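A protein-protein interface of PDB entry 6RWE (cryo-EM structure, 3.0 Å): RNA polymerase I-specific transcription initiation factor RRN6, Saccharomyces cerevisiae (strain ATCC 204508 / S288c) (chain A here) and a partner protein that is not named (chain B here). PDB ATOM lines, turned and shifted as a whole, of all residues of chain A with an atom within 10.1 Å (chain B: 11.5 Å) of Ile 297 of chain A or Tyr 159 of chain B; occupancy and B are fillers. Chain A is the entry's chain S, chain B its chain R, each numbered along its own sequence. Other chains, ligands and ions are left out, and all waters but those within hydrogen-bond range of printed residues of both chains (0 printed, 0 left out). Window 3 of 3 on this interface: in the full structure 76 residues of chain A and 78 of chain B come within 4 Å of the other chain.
O of Gly 322 of chain A lies within hydrogen-bond range of N of Phe 352 of chain A, 3.1 Å away.
No residue of chain B comes within 4 Å of Glu 296 of chain A. Of chain B, only Tyr 159 comes within 4 Å of Ile 297 of chain A. Asp 298 of chain A touches two residues of chain B. Of the printed residues of chain A, Lys 156 of chain B touches Asn 323. Of the printed residues of chain A, Met 157 of chain B touches Asn 323 (2.8 Å) and Phe 352 (3.6 Å). Of chain A, only Ile 297 (3.3 Å) and Asp 298 (3.2 Å) come within 4 Å of Tyr 159 of chain B. No residue of chain A comes within 4 Å of His 160 of chain B. The nearest residue of chain B that does not touch Ile 297 of chain A is Thr 158 of chain B (5.1 Å). The nearest residue of chain A that does not touch Tyr 159 of chain B is Glu 296 of chain A (6.2 Å). The nearest printed residue of chain B that does not touch Asn 323 of chain A is Thr 158 of chain B (4.5 Å).
Of the 17 printed residues of chain B, 5 touch a printed residue of chain A. Printed residues of chain B that touch a printed residue of chain A: Lys 156, Met 157, Thr 158, Tyr 159 and Phe 162. Of the 17 printed residues of chain A, 4 touch a printed residue of chain B. Printed residues of chain A that touch a printed residue of chain B: Ile 297, Asp 298, Asn 323 and Phe 352. Among the printed residues, 7 pairs touch across the chains. Among the printed residues, no Asp or Glu carboxylate lies within 4 Å of a Lys or Arg side-chain nitrogen of the other chain.
CB of Tyr 159 of chain B touches O of Ile 297 of chain A, at 3.3 Å. C of Thr 158 of chain B touches OD2 of Asp 298 of chain A, at 3.5 Å. Lys 156 of chain B touches Asn 323 of chain A. CE2 of Phe 352 of chain A touches CE of Met 157 of chain B (3.6 Å). CD1 of Phe 162 of chain B touches CZ of Phe 352 of chain A, 3.6 Å away.
N of Tyr 159 of chain B sits at hydrogen-bond distance from OD2 of Asp 298 of chain A, 3.2 Å away. O of Met 157 of chain B lies within hydrogen-bond range of ND2 of Asn 323 of chain A, at 2.8 Å.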
ATOM      1  N   GLU A 266     -15.605  23.362  28.397  1.00  0.00           N
ATOM      2  CA  GLU A 266     -14.989  22.375  27.523  1.00  0.00           C
ATOM      3  C   GLU A 266     -14.993  20.986  28.142  1.00  0.00           C
ATOM      4  O   GLU A 266     -14.866  19.995  27.416  1.00  0.00           O
ATOM      5  CB  GLU A 266     -13.547  22.785  27.222  1.00  0.00           C
ATOM      6  CG  GLU A 266     -13.400  24.101  26.486  1.00  0.00           C
ATOM      7  CD  GLU A 266     -11.948  24.534  26.363  1.00  0.00           C
ATOM      8  OE1 GLU A 266     -11.080  23.866  26.961  1.00  0.00           O
ATOM      9  OE2 GLU A 266     -11.673  25.545  25.681  1.00  0.00           O
ATOM     10  N   ASN A 267     -15.144  20.895  29.463  1.00  0.00           N
ATOM     11  CA  ASN A 267     -14.883  19.668  30.199  1.00  0.00           C
ATOM     12  C   ASN A 267     -16.055  19.165  31.025  1.00  0.00           C
ATOM     13  O   ASN A 267     -16.103  17.964  31.312  1.00  0.00           O
ATOM     14  CB  ASN A 267     -13.685  19.868  31.137  1.00  0.00           C
ATOM     15  CG  ASN A 267     -12.427  20.259  30.396  1.00  0.00           C
ATOM     16  OD1 ASN A 267     -11.934  21.380  30.531  1.00  0.00           O
ATOM     17  ND2 ASN A 267     -11.891  19.333  29.612  1.00  0.00           N
ATOM     18  N   SER A 268     -17.000  20.016  31.404  1.00  0.00           N
ATOM     19  CA  SER A 268     -17.975  19.642  32.417  1.00  0.00           C
ATOM     20  C   SER A 268     -19.289  20.351  32.121  1.00  0.00           C
ATOM     21  O   SER A 268     -19.500  20.861  31.015  1.00  0.00           O
ATOM     22  CB  SER A 268     -17.442  19.983  33.817  1.00  0.00           C
ATOM     23  OG  SER A 268     -17.319  21.387  33.978  1.00  0.00           O
ATOM     24  N   TYR A 293     -19.858  15.702  34.350  1.00  0.00           N
ATOM     25  CA  TYR A 293     -18.789  15.624  33.331  1.00  0.00           C
ATOM     26  C   TYR A 293     -19.270  14.803  32.139  1.00  0.00           C
ATOM     27  O   TYR A 293     -20.438  14.448  32.056  1.00  0.00           O
ATOM     28  CB  TYR A 293     -17.509  15.080  33.958  1.00  0.00           C
ATOM     29  CG  TYR A 293     -16.809  16.095  34.814  1.00  0.00           C
ATOM     30  CD1 TYR A 293     -15.986  17.045  34.245  1.00  0.00           C
ATOM     31  CD2 TYR A 293     -16.998  16.127  36.181  1.00  0.00           C
ATOM     32  CE1 TYR A 293     -15.353  17.995  35.021  1.00  0.00           C
ATOM     33  CE2 TYR A 293     -16.368  17.069  36.974  1.00  0.00           C
ATOM     34  CZ  TYR A 293     -15.539  18.005  36.388  1.00  0.00           C
ATOM     35  OH  TYR A 293     -14.905  18.938  37.148  1.00  0.00           O
ATOM     36  N   PHE A 294     -18.350  14.497  31.240  1.00  0.00           N
ATOM     37  CA  PHE A 294     -18.706  13.776  30.024  1.00  0.00           C
ATOM     38  C   PHE A 294     -18.635  12.285  30.323  1.00  0.00           C
ATOM     39  O   PHE A 294     -17.572  11.664  30.257  1.00  0.00           O
ATOM     40  CB  PHE A 294     -17.804  14.167  28.863  1.00  0.00           C
ATOM     41  CG  PHE A 294     -17.989  15.582  28.410  1.00  0.00           C
ATOM     42  CD1 PHE A 294     -19.175  15.974  27.813  1.00  0.00           C
ATOM     43  CD2 PHE A 294     -16.968  16.506  28.532  1.00  0.00           C
ATOM     44  CE1 PHE A 294     -19.357  17.276  27.387  1.00  0.00           C
ATOM     45  CE2 PHE A 294     -17.142  17.808  28.093  1.00  0.00           C
ATOM     46  CZ  PHE A 294     -18.336  18.192  27.521  1.00  0.00           C
ATOM     47  N   VAL A 295     -19.785  11.718  30.693  1.00  0.00           N
ATOM     48  CA  VAL A 295     -19.907  10.267  30.799  1.00  0.00           C
ATOM     49  C   VAL A 295     -19.732   9.634  29.426  1.00  0.00           C
ATOM     50  O   VAL A 295     -18.847   8.799  29.210  1.00  0.00           O
ATOM     51  CB  VAL A 295     -21.257   9.880  31.426  1.00  0.00           C
ATOM     52  CG1 VAL A 295     -21.412   8.365  31.445  1.00  0.00           C
ATOM     53  CG2 VAL A 295     -21.383  10.463  32.827  1.00  0.00           C
ATOM     54  N   GLU A 296     -20.584  10.021  28.482  1.00  0.00           N
ATOM     55  CA  GLU A 296     -20.265   9.869  27.073  1.00  0.00           C
ATOM     56  C   GLU A 296     -19.426  11.061  26.631  1.00  0.00           C
ATOM     57  O   GLU A 296     -19.696  12.206  27.006  1.00  0.00           O
ATOM     58  CB  GLU A 296     -21.544   9.725  26.237  1.00  0.00           C
ATOM     59  CG  GLU A 296     -22.527  10.889  26.292  1.00  0.00           C
ATOM     60  CD  GLU A 296     -23.534  10.762  27.422  1.00  0.00           C
ATOM     61  OE1 GLU A 296     -23.339   9.916  28.319  1.00  0.00           O
ATOM     62  OE2 GLU A 296     -24.525  11.519  27.420  1.00  0.00           O
ATOM     63  N   ILE A 297     -18.368  10.787  25.879  1.00  0.00           N
ATOM     64  CA  ILE A 297     -17.358  11.796  25.580  1.00  0.00           C
ATOM     65  C   ILE A 297     -17.682  12.340  24.194  1.00  0.00           C
ATOM     66  O   ILE A 297     -17.201  11.850  23.173  1.00  0.00           O
ATOM     67  CB  ILE A 297     -15.943  11.235  25.676  1.00  0.00           C
ATOM     68  CG1 ILE A 297     -15.719  10.614  27.054  1.00  0.00           C
ATOM     69  CG2 ILE A 297     -14.923  12.349  25.478  1.00  0.00           C
ATOM     70  CD1 ILE A 297     -14.448   9.799  27.156  1.00  0.00           C
ATOM     71  N   ASP A 298     -18.533  13.364  24.175  1.00  0.00           N
ATOM     72  CA  ASP A 298     -18.813  14.214  23.028  1.00  0.00           C
ATOM     73  C   ASP A 298     -19.169  15.584  23.578  1.00  0.00           C
ATOM     74  O   ASP A 298     -19.751  15.691  24.658  1.00  0.00           O
ATOM     75  CB  ASP A 298     -19.957  13.682  22.154  1.00  0.00           C
ATOM     76  CG  ASP A 298     -19.522  12.591  21.211  1.00  0.00           C
ATOM     77  OD1 ASP A 298     -18.381  12.652  20.711  1.00  0.00           O
ATOM     78  OD2 ASP A 298     -20.326  11.669  20.968  1.00  0.00           O
ATOM     79  N   ASP A 299     -18.808  16.627  22.842  1.00  0.00           N
ATOM     80  CA  ASP A 299     -18.986  17.985  23.343  1.00  0.00           C
ATOM     81  C   ASP A 299     -20.458  18.372  23.278  1.00  0.00           C
ATOM     82  O   ASP A 299     -21.073  18.331  22.208  1.00  0.00           O
ATOM     83  CB  ASP A 299     -18.134  18.957  22.532  1.00  0.00           C
ATOM     84  CG  ASP A 299     -18.021  20.332  23.178  1.00  0.00           C
ATOM     85  OD1 ASP A 299     -18.613  20.568  24.253  1.00  0.00           O
ATOM     86  OD2 ASP A 299     -17.318  21.188  22.605  1.00  0.00           O
ATOM     87  N   LEU A 300     -21.021  18.751  24.423  1.00  0.00           N
ATOM     88  CA  LEU A 300     -22.382  19.255  24.435  1.00  0.00           C
ATOM     89  C   LEU A 300     -22.425  20.643  23.810  1.00  0.00           C
ATOM     90  O   LEU A 300     -21.418  21.354  23.737  1.00  0.00           O
ATOM     91  CB  LEU A 300     -22.959  19.330  25.849  1.00  0.00           C
ATOM     92  CG  LEU A 300     -22.598  20.547  26.706  1.00  0.00           C
ATOM     93  CD1 LEU A 300     -23.649  20.747  27.776  1.00  0.00           C
ATOM     94  CD2 LEU A 300     -21.232  20.386  27.347  1.00  0.00           C
ATOM     95  N   GLN A 301     -23.613  21.027  23.348  1.00  0.00           N
ATOM     96  CA  GLN A 301     -23.752  22.274  22.611  1.00  0.00           C
ATOM     97  C   GLN A 301     -24.642  23.287  23.314  1.00  0.00           C
ATOM     98  O   GLN A 301     -24.185  24.397  23.603  1.00  0.00           O
ATOM     99  CB  GLN A 301     -24.279  21.969  21.208  1.00  0.00           C
ATOM    100  CG  GLN A 301     -23.324  21.114  20.415  1.00  0.00           C
ATOM    101  CD  GLN A 301     -22.000  21.809  20.203  1.00  0.00           C
ATOM    102  OE1 GLN A 301     -21.949  23.011  19.937  1.00  0.00           O
ATOM    103  NE2 GLN A 301     -20.915  21.063  20.343  1.00  0.00           N
ATOM    104  N   ILE A 320     -26.121  17.269  22.925  1.00  0.00           N
ATOM    105  CA  ILE A 320     -24.749  16.968  22.537  1.00  0.00           C
ATOM    106  C   ILE A 320     -24.740  16.895  21.008  1.00  0.00           C
ATOM    107  O   ILE A 320     -25.800  16.970  20.378  1.00  0.00           O
ATOM    108  CB  ILE A 320     -24.276  15.667  23.206  1.00  0.00           C
ATOM    109  CG1 ILE A 320     -24.751  15.629  24.652  1.00  0.00           C
ATOM    110  CG2 ILE A 320     -22.782  15.651  23.367  1.00  0.00           C
ATOM    111  CD1 ILE A 320     -24.574  14.279  25.317  1.00  0.00           C
ATOM    112  N   LYS A 321     -23.558  16.772  20.396  1.00  0.00           N
ATOM    113  CA  LYS A 321     -23.415  16.782  18.944  1.00  0.00           C
ATOM    114  C   LYS A 321     -24.062  15.578  18.278  1.00  0.00           C
ATOM    115  O   LYS A 321     -23.430  14.532  18.110  1.00  0.00           O
ATOM    116  CB  LYS A 321     -21.939  16.801  18.567  1.00  0.00           C
ATOM    117  CG  LYS A 321     -21.249  18.118  18.763  1.00  0.00           C
ATOM    118  CD  LYS A 321     -19.743  17.943  18.689  1.00  0.00           C
ATOM    119  CE  LYS A 321     -19.191  18.092  17.279  1.00  0.00           C
ATOM    120  NZ  LYS A 321     -19.447  16.924  16.385  1.00  0.00           N
ATOM    121  N   GLY A 322     -25.311  15.742  17.860  1.00  0.00           N
ATOM    122  CA  GLY A 322     -26.067  14.704  17.199  1.00  0.00           C
ATOM    123  C   GLY A 322     -27.166  14.105  18.041  1.00  0.00           C
ATOM    124  O   GLY A 322     -28.069  13.472  17.486  1.00  0.00           O
ATOM    125  N   ASN A 323     -27.141  14.311  19.355  1.00  0.00           N
ATOM    126  CA  ASN A 323     -28.019  13.591  20.263  1.00  0.00           C
ATOM    127  C   ASN A 323     -28.288  14.416  21.511  1.00  0.00           C
ATOM    128  O   ASN A 323     -27.449  15.204  21.947  1.00  0.00           O
ATOM    129  CB  ASN A 323     -27.413  12.238  20.620  1.00  0.00           C
ATOM    130  CG  ASN A 323     -25.954  12.337  21.014  1.00  0.00           C
ATOM    131  OD1 ASN A 323     -25.382  13.422  21.054  1.00  0.00           O
ATOM    132  ND2 ASN A 323     -25.336  11.198  21.292  1.00  0.00           N
ATOM    133  N   PHE A 352     -28.890  12.820  14.577  1.00  0.00           N
ATOM    134  CA  PHE A 352     -27.585  12.831  13.915  1.00  0.00           C
ATOM    135  C   PHE A 352     -27.639  12.620  12.406  1.00  0.00           C
ATOM    136  O   PHE A 352     -27.987  11.539  11.923  1.00  0.00           O
ATOM    137  CB  PHE A 352     -26.668  11.769  14.525  1.00  0.00           C
ATOM    138  CG  PHE A 352     -25.304  11.723  13.898  1.00  0.00           C
ATOM    139  CD1 PHE A 352     -24.361  12.688  14.200  1.00  0.00           C
ATOM    140  CD2 PHE A 352     -24.966  10.715  13.001  1.00  0.00           C
ATOM    141  CE1 PHE A 352     -23.107  12.653  13.625  1.00  0.00           C
ATOM    142  CE2 PHE A 352     -23.721  10.680  12.419  1.00  0.00           C
ATOM    143  CZ  PHE A 352     -22.788  11.648  12.732  1.00  0.00           C
ATOM    144  N   ILE B  34     -23.963   1.017   7.663  1.00  0.00           N
ATOM    145  CA  ILE B  34     -23.843   0.743   9.090  1.00  0.00           C
ATOM    146  C   ILE B  34     -25.193   0.942   9.774  1.00  0.00           C
ATOM    147  O   ILE B  34     -25.492   0.290  10.782  1.00  0.00           O
ATOM    148  CB  ILE B  34     -22.735   1.621   9.699  1.00  0.00           C
ATOM    149  CG1 ILE B  34     -21.424   1.432   8.930  1.00  0.00           C
ATOM    150  CG2 ILE B  34     -22.479   1.295  11.166  1.00  0.00           C
ATOM    151  CD1 ILE B  34     -20.906   0.020   8.898  1.00  0.00           C
ATOM    152  N   GLN B 155     -31.857   5.523  19.729  1.00  0.00           N
ATOM    153  CA  GLN B 155     -30.517   4.948  19.650  1.00  0.00           C
ATOM    154  C   GLN B 155     -29.571   6.037  19.173  1.00  0.00           C
ATOM    155  O   GLN B 155     -29.398   6.270  17.977  1.00  0.00           O
ATOM    156  CB  GLN B 155     -30.492   3.733  18.735  1.00  0.00           C
ATOM    157  CG  GLN B 155     -31.347   2.590  19.244  1.00  0.00           C
ATOM    158  CD  GLN B 155     -30.886   2.073  20.596  1.00  0.00           C
ATOM    159  OE1 GLN B 155     -29.690   1.989  20.868  1.00  0.00           O
ATOM    160  NE2 GLN B 155     -31.841   1.724  21.449  1.00  0.00           N
ATOM    161  N   LYS B 156     -28.948   6.705  20.137  1.00  0.00           N
ATOM    162  CA  LYS B 156     -28.147   7.876  19.845  1.00  0.00           C
ATOM    163  C   LYS B 156     -26.815   7.485  19.218  1.00  0.00           C
ATOM    164  O   LYS B 156     -26.447   6.310  19.130  1.00  0.00           O
ATOM    165  CB  LYS B 156     -27.909   8.693  21.108  1.00  0.00           C
ATOM    166  CG  LYS B 156     -27.071   8.020  22.166  1.00  0.00           C
ATOM    167  CD  LYS B 156     -26.881   8.963  23.342  1.00  0.00           C
ATOM    168  CE  LYS B 156     -26.076   8.322  24.456  1.00  0.00           C
ATOM    169  NZ  LYS B 156     -26.848   7.244  25.136  1.00  0.00           N
ATOM    170  N   MET B 157     -26.084   8.514  18.772  1.00  0.00           N
ATOM    171  CA  MET B 157     -24.750   8.359  18.131  1.00  0.00           C
ATOM    172  C   MET B 157     -23.678   8.873  19.092  1.00  0.00           C
ATOM    173  O   MET B 157     -23.674  10.078  19.386  1.00  0.00           O
ATOM    174  CB  MET B 157     -24.660   9.149  16.824  1.00  0.00           C
ATOM    175  CG  MET B 157     -24.369   8.275  15.628  1.00  0.00           C
ATOM    176  SD  MET B 157     -22.668   8.426  15.049  1.00  0.00           S
ATOM    177  CE  MET B 157     -22.747   7.420  13.571  1.00  0.00           C
ATOM    178  N   THR B 158     -22.799   7.974  19.535  1.00  0.00           N
ATOM    179  CA  THR B 158     -21.750   8.279  20.492  1.00  0.00           C
ATOM    180  C   THR B 158     -20.413   8.363  19.767  1.00  0.00           C
ATOM    181  O   THR B 158     -20.332   8.212  18.546  1.00  0.00           O
ATOM    182  CB  THR B 158     -21.709   7.228  21.603  1.00  0.00           C
ATOM    183  OG1 THR B 158     -20.769   7.630  22.609  1.00  0.00           O
ATOM    184  CG2 THR B 158     -21.305   5.872  21.035  1.00  0.00           C
ATOM    185  N   TYR B 159     -19.355   8.611  20.540  1.00  0.00           N
ATOM    186  CA  TYR B 159     -18.029   8.764  19.955  1.00  0.00           C
ATOM    187  C   TYR B 159     -17.475   7.438  19.450  1.00  0.00           C
ATOM    188  O   TYR B 159     -16.658   7.429  18.522  1.00  0.00           O
ATOM    189  CB  TYR B 159     -17.077   9.378  20.977  1.00  0.00           C
ATOM    190  CG  TYR B 159     -15.695   9.633  20.437  1.00  0.00           C
ATOM    191  CD1 TYR B 159     -15.454  10.699  19.586  1.00  0.00           C
ATOM    192  CD2 TYR B 159     -14.633   8.802  20.768  1.00  0.00           C
ATOM    193  CE1 TYR B 159     -14.193  10.940  19.084  1.00  0.00           C
ATOM    194  CE2 TYR B 159     -13.368   9.032  20.269  1.00  0.00           C
ATOM    195  CZ  TYR B 159     -13.154  10.105  19.428  1.00  0.00           C
ATOM    196  OH  TYR B 159     -11.898  10.345  18.924  1.00  0.00           O
ATOM    197  N   HIS B 160     -17.902   6.319  20.050  1.00  0.00           N
ATOM    198  CA  HIS B 160     -17.403   5.007  19.647  1.00  0.00           C
ATOM    199  C   HIS B 160     -17.827   4.660  18.228  1.00  0.00           C
ATOM    200  O   HIS B 160     -17.059   4.059  17.468  1.00  0.00           O
ATOM    201  CB  HIS B 160     -17.909   3.934  20.611  1.00  0.00           C
ATOM    202  CG  HIS B 160     -17.366   4.052  22.000  1.00  0.00           C
ATOM    203  ND1 HIS B 160     -17.964   4.827  22.970  1.00  0.00           N
ATOM    204  CD2 HIS B 160     -16.295   3.471  22.589  1.00  0.00           C
ATOM    205  CE1 HIS B 160     -17.275   4.729  24.094  1.00  0.00           C
ATOM    206  NE2 HIS B 160     -16.258   3.911  23.890  1.00  0.00           N
ATOM    207  N   ASN B 161     -19.046   5.030  17.854  1.00  0.00           N
ATOM    208  CA  ASN B 161     -19.544   4.748  16.517  1.00  0.00           C
ATOM    209  C   ASN B 161     -19.059   5.795  15.526  1.00  0.00           C
ATOM    210  O   ASN B 161     -18.799   5.482  14.360  1.00  0.00           O
ATOM    211  CB  ASN B 161     -21.070   4.705  16.535  1.00  0.00           C
ATOM    212  CG  ASN B 161     -21.602   3.622  17.436  1.00  0.00           C
ATOM    213  OD1 ASN B 161     -21.076   2.509  17.465  1.00  0.00           O
ATOM    214  ND2 ASN B 161     -22.645   3.943  18.194  1.00  0.00           N
ATOM    215  N   PHE B 162     -18.929   7.038  15.990  1.00  0.00           N
ATOM    216  CA  PHE B 162     -18.576   8.142  15.107  1.00  0.00           C
ATOM    217  C   PHE B 162     -17.113   8.071  14.687  1.00  0.00           C
ATOM    218  O   PHE B 162     -16.749   8.517  13.594  1.00  0.00           O
ATOM    219  CB  PHE B 162     -18.884   9.472  15.801  1.00  0.00           C
ATOM    220  CG  PHE B 162     -18.601  10.680  14.959  1.00  0.00           C
ATOM    221  CD1 PHE B 162     -19.437  11.016  13.905  1.00  0.00           C
ATOM    222  CD2 PHE B 162     -17.509  11.486  15.227  1.00  0.00           C
ATOM    223  CE1 PHE B 162     -19.182  12.127  13.127  1.00  0.00           C
ATOM    224  CE2 PHE B 162     -17.249  12.602  14.453  1.00  0.00           C
ATOM    225  CZ  PHE B 162     -18.087  12.921  13.400  1.00  0.00           C
ATOM    226  N   LYS B 163     -16.256   7.509  15.546  1.00  0.00           N
ATOM    227  CA  LYS B 163     -14.833   7.447  15.232  1.00  0.00           C
ATOM    228  C   LYS B 163     -14.527   6.430  14.139  1.00  0.00           C
ATOM    229  O   LYS B 163     -13.534   6.577  13.418  1.00  0.00           O
ATOM    230  CB  LYS B 163     -14.021   7.135  16.493  1.00  0.00           C
ATOM    231  CG  LYS B 163     -14.256   5.751  17.089  1.00  0.00           C
ATOM    232  CD  LYS B 163     -13.430   5.516  18.343  1.00  0.00           C
ATOM    233  CE  LYS B 163     -11.975   5.269  18.006  1.00  0.00           C
ATOM    234  NZ  LYS B 163     -11.816   3.981  17.277  1.00  0.00           N
ATOM    235  N   LYS B 164     -15.356   5.397  13.993  1.00  0.00           N
ATOM    236  CA  LYS B 164     -15.099   4.386  12.979  1.00  0.00           C
ATOM    237  C   LYS B 164     -15.831   4.657  11.679  1.00  0.00           C
ATOM    238  O   LYS B 164     -15.399   4.171  10.627  1.00  0.00           O
ATOM    239  CB  LYS B 164     -15.487   2.991  13.485  1.00  0.00           C
ATOM    240  CG  LYS B 164     -16.975   2.776  13.689  1.00  0.00           C
ATOM    241  CD  LYS B 164     -17.257   1.352  14.103  1.00  0.00           C
ATOM    242  CE  LYS B 164     -16.953   0.401  12.958  1.00  0.00           C
ATOM    243  NZ  LYS B 164     -17.857   0.620  11.798  1.00  0.00           N
ATOM    244  N   ILE B 165     -16.917   5.430  11.722  1.00  0.00           N
ATOM    245  CA  ILE B 165     -17.710   5.673  10.524  1.00  0.00           C
ATOM    246  C   ILE B 165     -17.084   6.752   9.657  1.00  0.00           C
ATOM    247  O   ILE B 165     -17.460   6.901   8.488  1.00  0.00           O
ATOM    248  CB  ILE B 165     -19.147   5.990  10.983  1.00  0.00           C
ATOM    249  CG1 ILE B 165     -20.155   5.741   9.869  1.00  0.00           C
ATOM    250  CG2 ILE B 165     -19.254   7.425  11.474  1.00  0.00           C
ATOM    251  CD1 ILE B 165     -21.550   5.625  10.365  1.00  0.00           C
ATOM    252  N   GLU B 166     -16.106   7.486  10.190  1.00  0.00           N
ATOM    253  CA  GLU B 166     -15.398   8.516   9.449  1.00  0.00           C
ATOM    254  C   GLU B 166     -13.962   8.142   9.120  1.00  0.00           C
ATOM    255  O   GLU B 166     -13.280   8.924   8.450  1.00  0.00           O
ATOM    256  CB  GLU B 166     -15.396   9.831  10.238  1.00  0.00           C
ATOM    257  CG  GLU B 166     -14.564   9.769  11.498  1.00  0.00           C
ATOM    258  CD  GLU B 166     -14.641  11.040  12.310  1.00  0.00           C
ATOM    259  OE1 GLU B 166     -15.353  11.973  11.882  1.00  0.00           O
ATOM    260  OE2 GLU B 166     -13.993  11.108  13.376  1.00  0.00           O
ATOM    261  N   LYS B 167     -13.484   6.979   9.568  1.00  0.00           N
ATOM    262  CA  LYS B 167     -12.098   6.601   9.313  1.00  0.00           C
ATOM    263  C   LYS B 167     -11.895   6.217   7.853  1.00  0.00           C
ATOM    264  O   LYS B 167     -11.069   6.811   7.152  1.00  0.00           O
ATOM    265  CB  LYS B 167     -11.687   5.450  10.228  1.00  0.00           C
ATOM    266  CG  LYS B 167     -10.228   5.044  10.079  1.00  0.00           C
ATOM    267  CD  LYS B 167      -9.857   3.919  11.032  1.00  0.00           C
ATOM    268  CE  LYS B 167     -10.443   2.588  10.565  1.00  0.00           C
ATOM    269  NZ  LYS B 167     -10.014   1.443  11.418  1.00  0.00           N
ATOM    270  N   LEU B 170     -12.131   9.143   5.448  1.00  0.00           N
ATOM    271  CA  LEU B 170     -10.953  10.011   5.478  1.00  0.00           C
ATOM    272  C   LEU B 170      -9.705   9.323   4.935  1.00  0.00           C
ATOM    273  O   LEU B 170      -8.819   9.994   4.393  1.00  0.00           O
ATOM    274  CB  LEU B 170     -10.697  10.511   6.897  1.00  0.00           C
ATOM    275  CG  LEU B 170     -11.612  11.623   7.402  1.00  0.00           C
ATOM    276  CD1 LEU B 170     -11.406  11.855   8.885  1.00  0.00           C
ATOM    277  CD2 LEU B 170     -11.306  12.887   6.629  1.00  0.00           C
ATOM    278  N   SER B 192     -13.956  19.409   8.564  1.00  0.00           N
ATOM    279  CA  SER B 192     -14.188  18.009   8.890  1.00  0.00           C
ATOM    280  C   SER B 192     -14.725  17.818  10.300  1.00  0.00           C
ATOM    281  O   SER B 192     -15.311  16.772  10.589  1.00  0.00           O
ATOM    282  CB  SER B 192     -12.896  17.216   8.722  1.00  0.00           C
ATOM    283  OG  SER B 192     -13.082  15.867   9.112  1.00  0.00           O
ATOM    284  N   ARG B 193     -14.559  18.804  11.177  1.00  0.00           N
ATOM    285  CA  ARG B 193     -14.857  18.648  12.595  1.00  0.00           C
ATOM    286  C   ARG B 193     -15.774  19.756  13.103  1.00  0.00           C
ATOM    287  O   ARG B 193     -15.775  20.076  14.295  1.00  0.00           O
ATOM    288  CB  ARG B 193     -13.558  18.601  13.397  1.00  0.00           C
ATOM    289  CG  ARG B 193     -12.709  19.857  13.262  1.00  0.00           C
ATOM    290  CD  ARG B 193     -11.409  19.728  14.026  1.00  0.00           C
ATOM    291  NE  ARG B 193     -10.535  18.725  13.428  1.00  0.00           N
ATOM    292  CZ  ARG B 193      -9.625  18.992  12.499  1.00  0.00           C
ATOM    293  NH1 ARG B 193      -9.461  20.235  12.067  1.00  0.00           N
ATOM    294  NH2 ARG B 193      -8.874  18.020  12.004  1.00  0.00           N
